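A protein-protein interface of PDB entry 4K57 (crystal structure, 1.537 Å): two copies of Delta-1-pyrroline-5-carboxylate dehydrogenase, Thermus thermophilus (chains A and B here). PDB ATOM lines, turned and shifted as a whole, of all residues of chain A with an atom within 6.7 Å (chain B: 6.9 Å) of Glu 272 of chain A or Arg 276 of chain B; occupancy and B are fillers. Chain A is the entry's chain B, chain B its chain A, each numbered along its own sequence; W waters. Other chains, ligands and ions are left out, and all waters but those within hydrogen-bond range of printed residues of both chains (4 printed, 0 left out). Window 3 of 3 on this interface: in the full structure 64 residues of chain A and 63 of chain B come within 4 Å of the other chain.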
ATOM      1  N   GLY A 267      12.057  16.586   7.039  1.00  0.00           N
ATOM      2  CA  GLY A 267      10.931  15.709   6.757  1.00  0.00           C
ATOM      3  C   GLY A 267      11.000  14.383   7.495  1.00  0.00           C
ATOM      4  O   GLY A 267       9.977  13.891   7.979  1.00  0.00           O
ATOM      5  N   LEU A 268      12.189  13.789   7.569  1.00  0.00           N
ATOM      6  CA  LEU A 268      12.356  12.543   8.309  1.00  0.00           C
ATOM      7  C   LEU A 268      12.002  12.714   9.786  1.00  0.00           C
ATOM      8  O   LEU A 268      11.332  11.860  10.373  1.00  0.00           O
ATOM      9  CB  LEU A 268      13.781  12.011   8.162  1.00  0.00           C
ATOM     10  CG  LEU A 268      14.174  11.474   6.794  1.00  0.00           C
ATOM     11  CD1 LEU A 268      15.686  11.241   6.739  1.00  0.00           C
ATOM     12  CD2 LEU A 268      13.421  10.190   6.483  1.00  0.00           C
ATOM     13  N   LYS A 269      12.446  13.821  10.378  1.00  0.00           N
ATOM     14  CA  LYS A 269      12.165  14.105  11.783  1.00  0.00           C
ATOM     15  C   LYS A 269      10.670  14.317  12.025  1.00  0.00           C
ATOM     16  O   LYS A 269      10.121  13.843  13.029  1.00  0.00           O
ATOM     17  CB  LYS A 269      12.955  15.333  12.248  1.00  0.00           C
ATOM     18  CG  LYS A 269      14.462  15.120  12.296  1.00  0.00           C
ATOM     19  CD  LYS A 269      15.192  16.420  12.639  1.00  0.00           C
ATOM     20  N   ILE A 270      10.017  15.032  11.113  1.00  0.00           N
ATOM     21  CA  ILE A 270       8.580  15.270  11.225  1.00  0.00           C
ATOM     22  C   ILE A 270       7.792  13.966  11.114  1.00  0.00           C
ATOM     23  O   ILE A 270       6.886  13.711  11.908  1.00  0.00           O
ATOM     24  CB  ILE A 270       8.084  16.284  10.174  1.00  0.00           C
ATOM     25  CG1 ILE A 270       8.580  17.684  10.534  1.00  0.00           C
ATOM     26  CG2 ILE A 270       6.558  16.263  10.071  1.00  0.00           C
ATOM     27  CD1 ILE A 270       8.328  18.701   9.446  1.00  0.00           C
ATOM     28  N   TYR A 271       8.150  13.130  10.147  1.00  0.00           N
ATOM     29  CA  TYR A 271       7.454  11.848   9.977  1.00  0.00           C
ATOM     30  C   TYR A 271       7.629  10.951  11.197  1.00  0.00           C
ATOM     31  O   TYR A 271       6.688  10.261  11.609  1.00  0.00           O
ATOM     32  CB  TYR A 271       7.941  11.132   8.713  1.00  0.00           C
ATOM     33  CG  TYR A 271       6.946  10.173   8.089  1.00  0.00           C
ATOM     34  CD1 TYR A 271       7.150   8.801   8.140  1.00  0.00           C
ATOM     35  CD2 TYR A 271       5.824  10.650   7.423  1.00  0.00           C
ATOM     36  CE1 TYR A 271       6.244   7.926   7.545  1.00  0.00           C
ATOM     37  CE2 TYR A 271       4.922   9.796   6.834  1.00  0.00           C
ATOM     38  CZ  TYR A 271       5.136   8.436   6.896  1.00  0.00           C
ATOM     39  OH  TYR A 271       4.228   7.595   6.297  1.00  0.00           O
ATOM     40  N   GLU A 272       8.829  10.946  11.778  1.00  0.00           N
ATOM     41  CA  GLU A 272       9.071  10.143  12.965  1.00  0.00           C
ATOM     42  C   GLU A 272       8.254  10.675  14.139  1.00  0.00           C
ATOM     43  O   GLU A 272       7.618   9.908  14.865  1.00  0.00           O
ATOM     44  CB  GLU A 272      10.563  10.092  13.306  1.00  0.00           C
ATOM     45  CG  GLU A 272      10.896   9.090  14.400  1.00  0.00           C
ATOM     46  CD  GLU A 272      12.384   8.899  14.606  1.00  0.00           C
ATOM     47  OE1 GLU A 272      13.157   9.073  13.641  1.00  0.00           O
ATOM     48  OE2 GLU A 272      12.778   8.573  15.740  1.00  0.00           O
ATOM     49  N   ALA A 273       8.257  11.993  14.314  1.00  0.00           N
ATOM     50  CA  ALA A 273       7.511  12.606  15.411  1.00  0.00           C
ATOM     51  C   ALA A 273       6.007  12.377  15.274  1.00  0.00           C
ATOM     52  O   ALA A 273       5.308  12.153  16.270  1.00  0.00           O
ATOM     53  CB  ALA A 273       7.826  14.102  15.505  1.00  0.00           C
ATOM     54  N   ALA A 274       5.514  12.428  14.041  1.00  0.00           N
ATOM     55  CA  ALA A 274       4.093  12.233  13.777  1.00  0.00           C
ATOM     56  C   ALA A 274       3.652  10.811  14.105  1.00  0.00           C
ATOM     57  O   ALA A 274       2.476  10.567  14.368  1.00  0.00           O
ATOM     58  CB  ALA A 274       3.765  12.577  12.340  1.00  0.00           C
ATOM     59  N   GLY A 275       4.596   9.876  14.089  1.00  0.00           N
ATOM     60  CA  GLY A 275       4.288   8.484  14.385  1.00  0.00           C
ATOM     61  C   GLY A 275       4.141   8.202  15.868  1.00  0.00           C
ATOM     62  O   GLY A 275       3.688   7.122  16.264  1.00  0.00           O
ATOM     63  N   ARG A 276       4.525   9.172  16.693  1.00  0.00           N
ATOM     64  CA  ARG A 276       4.523   9.006  18.138  1.00  0.00           C
ATOM     65  C   ARG A 276       3.235   9.514  18.766  1.00  0.00           C
ATOM     66  O   ARG A 276       2.638  10.478  18.284  1.00  0.00           O
ATOM     67  CB  ARG A 276       5.715   9.753  18.748  1.00  0.00           C
ATOM     68  CG  ARG A 276       7.065   9.172  18.370  1.00  0.00           C
ATOM     69  CD  ARG A 276       8.155   9.659  19.315  1.00  0.00           C
ATOM     70  NE  ARG A 276       8.119  11.108  19.466  1.00  0.00           N
ATOM     71  CZ  ARG A 276       8.905  11.957  18.809  1.00  0.00           C
ATOM     72  NH1 ARG A 276       8.783  13.263  19.015  1.00  0.00           N
ATOM     73  NH2 ARG A 276       9.807  11.510  17.943  1.00  0.00           N
ATOM     74  N   VAL B 250       7.919  -5.437  10.577  1.00  0.00           N
ATOM     75  CA  VAL B 250       7.513  -4.035  10.712  1.00  0.00           C
ATOM     76  C   VAL B 250       8.710  -3.074  10.618  1.00  0.00           C
ATOM     77  O   VAL B 250       8.630  -2.025   9.957  1.00  0.00           O
ATOM     78  CB  VAL B 250       6.738  -3.800  12.031  1.00  0.00           C
ATOM     79  CG1 VAL B 250       6.623  -2.314  12.340  1.00  0.00           C
ATOM     80  CG2 VAL B 250       5.367  -4.439  11.967  1.00  0.00           C
ATOM     81  N   GLU B 251       9.823  -3.444  11.251  1.00  0.00           N
ATOM     82  CA  GLU B 251      11.010  -2.588  11.329  1.00  0.00           C
ATOM     83  C   GLU B 251      11.974  -2.715  10.143  1.00  0.00           C
ATOM     84  O   GLU B 251      12.917  -1.929  10.012  1.00  0.00           O
ATOM     85  CB  GLU B 251      11.758  -2.857  12.640  1.00  0.00           C
ATOM     86  CG  GLU B 251      10.922  -2.584  13.888  1.00  0.00           C
ATOM     87  CD  GLU B 251      11.551  -3.121  15.165  1.00  0.00           C
ATOM     88  OE1 GLU B 251      12.569  -3.849  15.086  1.00  0.00           O
ATOM     89  OE2 GLU B 251      11.016  -2.819  16.253  1.00  0.00           O
ATOM     90  N   LYS B 269       2.675   0.845  18.726  1.00  0.00           N
ATOM     91  CA  LYS B 269       4.064   0.487  18.476  1.00  0.00           C
ATOM     92  C   LYS B 269       4.367   0.391  16.984  1.00  0.00           C
ATOM     93  O   LYS B 269       5.443   0.802  16.535  1.00  0.00           O
ATOM     94  CB  LYS B 269       4.400  -0.834  19.168  1.00  0.00           C
ATOM     95  CG  LYS B 269       4.381  -0.740  20.680  1.00  0.00           C
ATOM     96  CD  LYS B 269       4.669  -2.091  21.320  1.00  0.00           C
ATOM     97  CE  LYS B 269       4.658  -1.986  22.836  1.00  0.00           C
ATOM     98  NZ  LYS B 269       4.839  -3.320  23.492  1.00  0.00           N
ATOM     99  N   TYR B 271       2.697   1.921  14.445  1.00  0.00           N
ATOM    100  CA  TYR B 271       2.660   3.256  13.849  1.00  0.00           C
ATOM    101  C   TYR B 271       3.941   4.019  14.155  1.00  0.00           C
ATOM    102  O   TYR B 271       4.479   4.705  13.283  1.00  0.00           O
ATOM    103  CB  TYR B 271       1.441   4.032  14.355  1.00  0.00           C
ATOM    104  CG  TYR B 271       0.927   5.121  13.429  1.00  0.00           C
ATOM    105  CD1 TYR B 271       1.024   6.463  13.778  1.00  0.00           C
ATOM    106  CD2 TYR B 271       0.312   4.799  12.233  1.00  0.00           C
ATOM    107  CE1 TYR B 271       0.529   7.460  12.936  1.00  0.00           C
ATOM    108  CE2 TYR B 271      -0.181   5.776  11.384  1.00  0.00           C
ATOM    109  CZ  TYR B 271      -0.073   7.099  11.742  1.00  0.00           C
ATOM    110  OH  TYR B 271      -0.578   8.054  10.890  1.00  0.00           O
ATOM    111  N   GLU B 272       4.441   3.908  15.388  1.00  0.00           N
ATOM    112  CA  GLU B 272       5.678   4.577  15.745  1.00  0.00           C
ATOM    113  C   GLU B 272       6.850   4.003  14.945  1.00  0.00           C
ATOM    114  O   GLU B 272       7.669   4.746  14.408  1.00  0.00           O
ATOM    115  CB  GLU B 272       5.941   4.497  17.256  1.00  0.00           C
ATOM    116  CG  GLU B 272       7.168   5.275  17.692  1.00  0.00           C
ATOM    117  CD  GLU B 272       7.331   5.362  19.201  1.00  0.00           C
ATOM    118  OE1 GLU B 272       6.326   5.227  19.931  1.00  0.00           O
ATOM    119  OE2 GLU B 272       8.473   5.569  19.650  1.00  0.00           O
ATOM    120  N   ALA B 273       6.924   2.681  14.856  1.00  0.00           N
ATOM    121  CA  ALA B 273       8.007   2.043  14.116  1.00  0.00           C
ATOM    122  C   ALA B 273       7.964   2.408  12.632  1.00  0.00           C
ATOM    123  O   ALA B 273       9.009   2.627  12.015  1.00  0.00           O
ATOM    124  CB  ALA B 273       7.959   0.525  14.301  1.00  0.00           C
ATOM    125  N   ALA B 274       6.754   2.483  12.078  1.00  0.00           N
ATOM    126  CA  ALA B 274       6.560   2.806  10.662  1.00  0.00           C
ATOM    127  C   ALA B 274       7.042   4.218  10.348  1.00  0.00           C
ATOM    128  O   ALA B 274       7.402   4.516   9.205  1.00  0.00           O
ATOM    129  CB  ALA B 274       5.119   2.643  10.262  1.00  0.00           C
ATOM    130  N   GLY B 275       7.045   5.086  11.357  1.00  0.00           N
ATOM    131  CA  GLY B 275       7.485   6.466  11.178  1.00  0.00           C
ATOM    132  C   GLY B 275       8.990   6.647  11.138  1.00  0.00           C
ATOM    133  O   GLY B 275       9.489   7.729  10.800  1.00  0.00           O
ATOM    134  N   ARG B 276       9.724   5.592  11.494  1.00  0.00           N
ATOM    135  CA  ARG B 276      11.176   5.647  11.548  1.00  0.00           C
ATOM    136  C   ARG B 276      11.799   5.156  10.249  1.00  0.00           C
ATOM    137  O   ARG B 276      11.253   4.267   9.583  1.00  0.00           O
ATOM    138  CB  ARG B 276      11.710   4.807  12.720  1.00  0.00           C
ATOM    139  CG  ARG B 276      11.211   5.239  14.096  1.00  0.00           C
ATOM    140  CD  ARG B 276      12.007   4.569  15.213  1.00  0.00           C
ATOM    141  NE  ARG B 276      11.919   3.110  15.155  1.00  0.00           N
ATOM    142  CZ  ARG B 276      11.137   2.365  15.933  1.00  0.00           C
ATOM    143  NH1 ARG B 276      11.129   1.046  15.795  1.00  0.00           N
ATOM    144  NH2 ARG B 276      10.363   2.932  16.852  1.00  0.00           N
ATOM    145  N   LEU B 277      12.943   5.738   9.898  1.00  0.00           N
ATOM    146  CA  LEU B 277      13.716   5.283   8.748  1.00  0.00           C
ATOM    147  C   LEU B 277      14.740   4.251   9.219  1.00  0.00           C
ATOM    148  O   LEU B 277      15.757   4.600   9.814  1.00  0.00           O
ATOM    149  CB  LEU B 277      14.444   6.461   8.082  1.00  0.00           C
ATOM    150  CG  LEU B 277      15.134   6.177   6.744  1.00  0.00           C
ATOM    151  CD1 LEU B 277      14.106   6.138   5.612  1.00  0.00           C
ATOM    152  CD2 LEU B 277      16.228   7.199   6.460  1.00  0.00           C
ATOM    153  N   ALA B 278      14.454   2.976   8.971  1.00  0.00           N
ATOM    154  CA  ALA B 278      15.420   1.920   9.260  1.00  0.00           C
ATOM    155  C   ALA B 278      16.676   2.148   8.433  1.00  0.00           C
ATOM    156  O   ALA B 278      16.613   2.750   7.363  1.00  0.00           O
ATOM    157  CB  ALA B 278      14.811   0.558   8.946  1.00  0.00           C
ATOM    158  N   GLN B 281      16.810   2.160   4.504  1.00  0.00           N
ATOM    159  CA  GLN B 281      15.445   2.298   3.990  1.00  0.00           C
ATOM    160  C   GLN B 281      15.359   3.466   3.000  1.00  0.00           C
ATOM    161  O   GLN B 281      16.009   4.490   3.194  1.00  0.00           O
ATOM    162  CB  GLN B 281      14.482   2.493   5.171  1.00  0.00           C
ATOM    163  CG  GLN B 281      12.997   2.615   4.848  1.00  0.00           C
ATOM    164  CD  GLN B 281      12.170   2.707   6.121  1.00  0.00           C
ATOM    165  OE1 GLN B 281      12.388   1.947   7.069  1.00  0.00           O
ATOM    166  NE2 GLN B 281      11.232   3.643   6.159  1.00  0.00           N
ATOM    167  N   TRP B 283      12.243   4.727   1.558  1.00  0.00           N
ATOM    168  CA  TRP B 283      10.900   5.278   1.404  1.00  0.00           C
ATOM    169  C   TRP B 283      10.303   5.623   2.753  1.00  0.00           C
ATOM    170  O   TRP B 283      10.853   5.257   3.802  1.00  0.00           O
ATOM    171  CB  TRP B 283       9.978   4.293   0.682  1.00  0.00           C
ATOM    172  CG  TRP B 283       9.977   2.895   1.274  1.00  0.00           C
ATOM    173  CD1 TRP B 283       9.506   2.515   2.500  1.00  0.00           C
ATOM    174  CD2 TRP B 283      10.460   1.706   0.639  1.00  0.00           C
ATOM    175  NE1 TRP B 283       9.671   1.152   2.666  1.00  0.00           N
ATOM    176  CE2 TRP B 283      10.259   0.637   1.540  1.00  0.00           C
ATOM    177  CE3 TRP B 283      11.047   1.440  -0.599  1.00  0.00           C
ATOM    178  CZ2 TRP B 283      10.620  -0.679   1.233  1.00  0.00           C
ATOM    179  CZ3 TRP B 283      11.409   0.132  -0.905  1.00  0.00           C
ATOM    180  CH2 TRP B 283      11.194  -0.912   0.010  1.00  0.00           C
ATOM    181  N   PHE B 284       9.176   6.329   2.711  1.00  0.00           N
ATOM    182  CA  PHE B 284       8.368   6.571   3.894  1.00  0.00           C
ATOM    183  C   PHE B 284       7.315   5.465   3.978  1.00  0.00           C
ATOM    184  O   PHE B 284       6.442   5.361   3.121  1.00  0.00           O
ATOM    185  CB  PHE B 284       7.712   7.963   3.818  1.00  0.00           C
ATOM    186  CG  PHE B 284       8.692   9.105   3.918  1.00  0.00           C
ATOM    187  CD1 PHE B 284       9.379   9.556   2.794  1.00  0.00           C
ATOM    188  CD2 PHE B 284       8.940   9.727   5.138  1.00  0.00           C
ATOM    189  CE1 PHE B 284      10.289  10.609   2.890  1.00  0.00           C
ATOM    190  CE2 PHE B 284       9.840  10.776   5.242  1.00  0.00           C
ATOM    191  CZ  PHE B 284      10.523  11.217   4.117  1.00  0.00           C
ATOM    192  N   LYS B 285       7.419   4.622   5.002  1.00  0.00           N
ATOM    193  CA  LYS B 285       6.483   3.511   5.158  1.00  0.00           C
ATOM    194  C   LYS B 285       5.058   4.003   5.354  1.00  0.00           C
ATOM    195  O   LYS B 285       4.836   5.020   6.026  1.00  0.00           O
ATOM    196  CB  LYS B 285       6.865   2.640   6.355  1.00  0.00           C
ATOM    197  CG  LYS B 285       8.049   1.738   6.098  1.00  0.00           C
ATOM    198  CD  LYS B 285       8.515   1.038   7.376  1.00  0.00           C
ATOM    199  CE  LYS B 285       9.694   0.145   7.066  1.00  0.00           C
ATOM    200  NZ  LYS B 285      10.291  -0.416   8.308  1.00  0.00           N
HETATM  201  O   HOH W   1       9.952   7.147  17.164  1.00  0.00           O
HETATM  202  O   HOH W   2       8.281   7.223  15.272  1.00  0.00           O
HETATM  203  O   HOH W   3      11.253   9.151   9.480  1.00  0.00           O
HETATM  204  O   HOH W   4      13.562   8.433  10.931  1.00  0.00           O
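O of Val 250 of chain B is in hydrogen-bond range of NZ of Lys 285 of chain B, 2.8 Å away. NZ of Lys 285 of chain B lies close to OE1 of Gln 281 of chain B (3.4 Å). OE2 of Glu 251 of chain B is in salt-bridge range of NH1 of Arg 276 of chain B (3.9 Å). The backbone carbonyl oxygen (O) of Glu 251 of chain B sits close to the side-chain amino group (NZ) of Lys 285 of chain B (3.5 Å). O of Arg 276 of chain B sits at hydrogen-bond distance from NE2 of Gln 281 of chain B (3.5 Å).
Among the printed residues, pairs that only touch across the chains: Leu 268 of chain A with Phe 284 of chain B (3.8 Å), Tyr 271 of chain A with Ala 274 of chain B (3.97 Å), Tyr 271 of chain A with Gly 275 of chain B (3.7 Å), Tyr 271 of chain A with Phe 284 of chain B (3.6 Å), Glu 272 of chain A with Arg 276 of chain B (3.9 Å), Ala 274 of chain A with Tyr 271 of chain B (3.9 Å), Gly 275 of chain A with Tyr 271 of chain B (3.7 Å) and Arg 276 of chain A with Glu 272 of chain B (3.9 Å).
Water W3 lies within hydrogen-bond range of O of Gly 275 of chain B and O of Leu 268 of chain A. Water W2 bridges the backbone carbonyl oxygen (O) of Glu 272 of chain B and the backbone carbonyl oxygen (O) of Glu 272 of chain A. Water W4 lies within hydrogen-bond range of OE1 of Glu 272 of chain A (2.8 Å) and N of Leu 277 of chain B (3.0 Å). Water W1 lies within hydrogen-bond range of OE2 of Glu 272 of chain B (3.3 Å) and OE2 of Glu 272 of chain A (3.5 Å).
O of Lys 285 of chain B sits at hydrogen-bond distance from OH of Tyr 271 of chain A (2.7 Å). O of Gly 275 of chain A sits close to N of Glu 272 of chain B (3.4 Å). The backbone carbonyl oxygen (O) of Gly 275 of chain B sits close to the backbone NH (N) of Glu 272 of chain A (3.4 Å).
Tyr 271 of chain A touches Ala 274 of chain B, and with the chains exchanged Ala 274 of chain A touches Tyr 271 of chain B. Tyr 271 of chain A touches Gly 275 of chain B, and with the chains exchanged Gly 275 of chain A touches Tyr 271 of chain B. Glu 272 of chain A touches Gly 275 of chain B, and with the chains exchanged Gly 275 of chain A touches Glu 272 of chain B. Glu 272 of chain A touches Arg 276 of chain B, and with the chains exchanged Arg 276 of chain A touches Glu 272 of chain B. Of the 11 pairs that touch across the chains among the printed residues, 8 have their exchanged pair printed and touching as well.
Of chain B, only Gly 275 (3.3 Å) and Arg 276 (3.9 Å) come within 4 Å of Glu 272 of chain A. Printed residues of chain B within 4 Å of Gly 275 of chain A: Tyr 271 (3.7 Å) and Glu 272 (3.3 Å). Of the printed residues of chain B, Ala 274 of chain A touches Tyr 271. Of the printed residues of chain B, Leu 268 of chain A touches Phe 284 (3.8 Å). Of the printed residues of chain A, Glu 272 of chain B touches Gly 275 and Arg 276. Printed residues of chain B within 4 Å of Tyr 271 of chain A: Ala 274, Gly 275, Phe 284 and Lys 285. Ala 273 of chain B touches none of the printed residues of chain A. Val 250 of chain B touches none of the printed residues of chain A. The nearest residue of chain B that does not touch Glu 272 of chain A is Leu 277 of chain B (5.0 Å). The nearest residue of chain A that does not touch Arg 276 of chain B is Tyr 271 of chain A (5.3 Å).
Of the 15 printed residues of chain B, 7 touch a printed residue of chain A. Printed residues of chain B that touch a printed residue of chain A: Tyr 271, Glu 272, Ala 274, Gly 275, Arg 276, Phe 284 and Lys 285. Hydrophobic or aromatic side chains of chain B that line the printed part of chain A: Tyr 271 and Phe 284. Of the 10 printed residues of chain A, 6 touch a printed residue of chain B. Among the printed residues, 11 pairs touch across the chains. Among the printed residues, no Asp or Glu carboxylate lies within 4 Å of a Lys or Arg side-chain nitrogen of the other chain.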
